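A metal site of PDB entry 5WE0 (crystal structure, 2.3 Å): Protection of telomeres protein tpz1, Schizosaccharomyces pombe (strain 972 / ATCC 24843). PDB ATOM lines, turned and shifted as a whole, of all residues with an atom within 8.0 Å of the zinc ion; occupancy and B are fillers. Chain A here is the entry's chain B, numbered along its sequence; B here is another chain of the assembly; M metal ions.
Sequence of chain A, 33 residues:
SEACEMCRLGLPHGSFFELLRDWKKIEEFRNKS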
ATOM      1  N   ALA A   3     -18.439 -10.222   1.517  1.00  0.00           N
ATOM      2  CA  ALA A   3     -17.960 -11.599   1.442  1.00  0.00           C
ATOM      3  C   ALA A   3     -16.646 -11.782   2.217  1.00  0.00           C
ATOM      4  O   ALA A   3     -15.647 -12.223   1.652  1.00  0.00           O
ATOM      5  CB  ALA A   3     -17.771 -12.009  -0.030  1.00  0.00           C
ATOM      6  N   CYS A   4     -16.657 -11.477   3.509  1.00  0.00           N
ATOM      7  CA  CYS A   4     -15.431 -11.341   4.300  1.00  0.00           C
ATOM      8  C   CYS A   4     -15.268 -12.481   5.297  1.00  0.00           C
ATOM      9  O   CYS A   4     -16.134 -12.729   6.137  1.00  0.00           O
ATOM     10  CB  CYS A   4     -15.416 -10.004   5.024  1.00  0.00           C
ATOM     11  SG  CYS A   4     -13.987  -9.808   6.073  1.00  0.00           S
ATOM     12  N   GLU A   5     -14.093 -13.142   5.233  1.00  0.00           N
ATOM     13  CA  GLU A   5     -13.812 -14.313   6.056  1.00  0.00           C
ATOM     14  C   GLU A   5     -13.719 -13.960   7.544  1.00  0.00           C
ATOM     15  O   GLU A   5     -14.297 -14.650   8.392  1.00  0.00           O
ATOM     16  CB  GLU A   5     -12.516 -14.979   5.564  1.00  0.00           C
ATOM     17  CG  GLU A   5     -11.985 -16.071   6.485  1.00  0.00           C
ATOM     18  CD  GLU A   5     -11.393 -17.265   5.727  1.00  0.00           C
ATOM     19  OE1 GLU A   5     -12.156 -18.222   5.439  1.00  0.00           O
ATOM     20  OE2 GLU A   5     -10.171 -17.246   5.418  1.00  0.00           O
ATOM     21  N   MET A   6     -12.982 -12.892   7.882  1.00  0.00           N
ATOM     22  CA  MET A   6     -12.930 -12.449   9.276  1.00  0.00           C
ATOM     23  C   MET A   6     -14.310 -12.066   9.816  1.00  0.00           C
ATOM     24  O   MET A   6     -14.601 -12.290  10.995  1.00  0.00           O
ATOM     25  CB  MET A   6     -11.944 -11.278   9.411  1.00  0.00           C
ATOM     26  CG  MET A   6     -10.578 -11.538   8.796  1.00  0.00           C
ATOM     27  SD  MET A   6      -9.628 -12.600   9.889  1.00  0.00           S
ATOM     28  CE  MET A   6      -9.417 -11.510  11.300  1.00  0.00           C
ATOM     29  N   CYS A   7     -15.200 -11.529   8.956  1.00  0.00           N
ATOM     30  CA  CYS A   7     -16.569 -11.279   9.393  1.00  0.00           C
ATOM     31  C   CYS A   7     -17.299 -12.575   9.672  1.00  0.00           C
ATOM     32  O   CYS A   7     -17.966 -12.714  10.705  1.00  0.00           O
ATOM     33  CB  CYS A   7     -17.326 -10.467   8.338  1.00  0.00           C
ATOM     34  SG  CYS A   7     -17.084  -8.712   8.517  1.00  0.00           S
ATOM     35  N   ARG A   8     -17.144 -13.560   8.779  1.00  0.00           N
ATOM     36  CA  ARG A   8     -17.835 -14.831   8.938  1.00  0.00           C
ATOM     37  C   ARG A   8     -17.297 -15.586  10.158  1.00  0.00           C
ATOM     38  O   ARG A   8     -18.050 -16.302  10.835  1.00  0.00           O
ATOM     39  CB  ARG A   8     -17.669 -15.647   7.647  1.00  0.00           C
ATOM     40  CG  ARG A   8     -18.655 -16.776   7.453  1.00  0.00           C
ATOM     41  CD  ARG A   8     -18.297 -17.671   6.255  1.00  0.00           C
ATOM     42  NE  ARG A   8     -16.882 -18.044   6.284  1.00  0.00           N
ATOM     43  CZ  ARG A   8     -16.421 -19.145   6.871  1.00  0.00           C
ATOM     44  NH1 ARG A   8     -17.261 -19.968   7.503  1.00  0.00           N
ATOM     45  NH2 ARG A   8     -15.115 -19.417   6.858  1.00  0.00           N
ATOM     46  N   LEU A   9     -16.015 -15.396  10.476  1.00  0.00           N
ATOM     47  CA  LEU A   9     -15.373 -16.017  11.622  1.00  0.00           C
ATOM     48  C   LEU A   9     -15.556 -15.238  12.922  1.00  0.00           C
ATOM     49  O   LEU A   9     -15.150 -15.737  13.977  1.00  0.00           O
ATOM     50  CB  LEU A   9     -13.883 -16.191  11.330  1.00  0.00           C
ATOM     51  CG  LEU A   9     -13.527 -17.176  10.212  1.00  0.00           C
ATOM     52  CD1 LEU A   9     -12.029 -17.379  10.113  1.00  0.00           C
ATOM     53  CD2 LEU A   9     -14.236 -18.506  10.455  1.00  0.00           C
ATOM     54  N   GLY A  10     -16.137 -14.038  12.896  1.00  0.00           N
ATOM     55  CA  GLY A  10     -16.329 -13.289  14.125  1.00  0.00           C
ATOM     56  C   GLY A  10     -15.068 -12.727  14.742  1.00  0.00           C
ATOM     57  O   GLY A  10     -15.070 -12.386  15.933  1.00  0.00           O
ATOM     58  N   LEU A  11     -13.930 -12.642  13.953  1.00  0.00           N
ATOM     59  CA  LEU A  11     -12.620 -12.184  14.424  1.00  0.00           C
ATOM     60  C   LEU A  11     -12.479 -10.676  14.272  1.00  0.00           C
ATOM     61  O   LEU A  11     -13.036 -10.088  13.346  1.00  0.00           O
ATOM     62  CB  LEU A  11     -11.508 -12.891  13.651  1.00  0.00           C
ATOM     63  CG  LEU A  11     -11.361 -14.410  13.857  1.00  0.00           C
ATOM     64  CD1 LEU A  11     -10.357 -14.992  12.877  1.00  0.00           C
ATOM     65  CD2 LEU A  11     -10.985 -14.749  15.290  1.00  0.00           C
ATOM     66  N   PRO A  12     -11.746 -10.004  15.165  1.00  0.00           N
ATOM     67  CA  PRO A  12     -11.525  -8.566  14.999  1.00  0.00           C
ATOM     68  C   PRO A  12     -10.603  -8.282  13.816  1.00  0.00           C
ATOM     69  O   PRO A  12      -9.644  -9.020  13.565  1.00  0.00           O
ATOM     70  CB  PRO A  12     -10.897  -8.139  16.332  1.00  0.00           C
ATOM     71  CG  PRO A  12     -10.257  -9.387  16.867  1.00  0.00           C
ATOM     72  CD  PRO A  12     -11.151 -10.514  16.421  1.00  0.00           C
ATOM     73  N   HIS A  13     -10.939  -7.229  13.064  1.00  0.00           N
ATOM     74  CA  HIS A  13     -10.227  -6.802  11.858  1.00  0.00           C
ATOM     75  C   HIS A  13     -10.766  -5.433  11.456  1.00  0.00           C
ATOM     76  O   HIS A  13     -11.766  -4.952  11.983  1.00  0.00           O
ATOM     77  CB  HIS A  13     -10.406  -7.805  10.704  1.00  0.00           C
ATOM     78  CG  HIS A  13     -11.840  -8.006  10.318  1.00  0.00           C
ATOM     79  ND1 HIS A  13     -12.770  -8.528  11.186  1.00  0.00           N
ATOM     80  CD2 HIS A  13     -12.501  -7.743   9.168  1.00  0.00           C
ATOM     81  CE1 HIS A  13     -13.947  -8.593  10.586  1.00  0.00           C
ATOM     82  NE2 HIS A  13     -13.813  -8.121   9.361  1.00  0.00           N
ATOM     83  N   GLY A  14     -10.103  -4.830  10.468  1.00  0.00           N
ATOM     84  CA  GLY A  14     -10.518  -3.544   9.948  1.00  0.00           C
ATOM     85  C   GLY A  14      -9.796  -2.378  10.603  1.00  0.00           C
ATOM     86  O   GLY A  14      -9.001  -2.530  11.541  1.00  0.00           O
ATOM     87  N   LYS B  45     -18.393  -5.501  15.786  1.00  0.00           N
ATOM     88  CA  LYS B  45     -18.578  -6.168  14.501  1.00  0.00           C
ATOM     89  C   LYS B  45     -19.178  -5.256  13.425  1.00  0.00           C
ATOM     90  O   LYS B  45     -18.983  -5.484  12.232  1.00  0.00           O
ATOM     91  CB  LYS B  45     -19.450  -7.412  14.668  1.00  0.00           C
ATOM     92  CG  LYS B  45     -18.759  -8.597  15.330  1.00  0.00           C
ATOM     93  CD  LYS B  45     -18.903  -8.552  16.846  1.00  0.00           C
ATOM     94  CE  LYS B  45     -18.539  -9.883  17.478  1.00  0.00           C
ATOM     95  NZ  LYS B  45     -18.801  -9.860  18.952  1.00  0.00           N
ATOM     96  N   MET B  47     -18.417  -2.116  12.874  1.00  0.00           N
ATOM     97  CA  MET B  47     -17.470  -1.101  12.416  1.00  0.00           C
ATOM     98  C   MET B  47     -16.353  -1.675  11.548  1.00  0.00           C
ATOM     99  O   MET B  47     -15.494  -0.920  11.094  1.00  0.00           O
ATOM    100  CB  MET B  47     -16.876  -0.351  13.613  1.00  0.00           C
ATOM    101  CG  MET B  47     -17.922   0.362  14.462  1.00  0.00           C
ATOM    102  SD  MET B  47     -18.894   1.525  13.491  1.00  0.00           S
ATOM    103  CE  MET B  47     -17.823   2.957  13.419  1.00  0.00           C
ATOM    104  N   CYS B  48     -16.346  -2.998  11.319  1.00  0.00           N
ATOM    105  CA  CYS B  48     -15.208  -3.634  10.662  1.00  0.00           C
ATOM    106  C   CYS B  48     -14.954  -3.058   9.269  1.00  0.00           C
ATOM    107  O   CYS B  48     -13.798  -2.939   8.855  1.00  0.00           O
ATOM    108  CB  CYS B  48     -15.428  -5.143  10.597  1.00  0.00           C
ATOM    109  SG  CYS B  48     -15.202  -5.928  12.207  1.00  0.00           S
ATOM    110  N   HIS B  49     -16.005  -2.669   8.547  1.00  0.00           N
ATOM    111  CA  HIS B  49     -15.855  -2.123   7.198  1.00  0.00           C
ATOM    112  C   HIS B  49     -16.371  -0.703   7.087  1.00  0.00           C
ATOM    113  O   HIS B  49     -16.601  -0.208   5.980  1.00  0.00           O
ATOM    114  CB  HIS B  49     -16.534  -3.031   6.179  1.00  0.00           C
ATOM    115  CG  HIS B  49     -15.943  -4.404   6.162  1.00  0.00           C
ATOM    116  ND1 HIS B  49     -14.724  -4.675   5.593  1.00  0.00           N
ATOM    117  CD2 HIS B  49     -16.352  -5.555   6.749  1.00  0.00           C
ATOM    118  CE1 HIS B  49     -14.422  -5.946   5.767  1.00  0.00           C
ATOM    119  NE2 HIS B  49     -15.399  -6.503   6.465  1.00  0.00           N
HETATM  120 ZN    ZN M   1     -14.966  -8.190   7.627  1.00  0.00          ZN
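SG of Cys 48 of chain B lies close to O of His 13 (3.6 Å). The backbone carbonyl oxygen of Leu 11 sits at hydrogen-bond distance from a ring nitrogen (ND1) of His 13, 2.7 Å away. The side-chain sulfur (SG) of Cys 4 sits close to the backbone NH (N) of Met 6, at 3.7 Å.
The nearest printed residue that does not touch the zinc ion is Cys 48 of chain B (4.3 Å).
The zinc ion is bound by NE2 of His 13 (2.1 Å), NE2 of His 49 of chain B (2.1 Å), SG of Cys 7 (2.4 Å) and SG of Cys 4 (2.4 Å).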
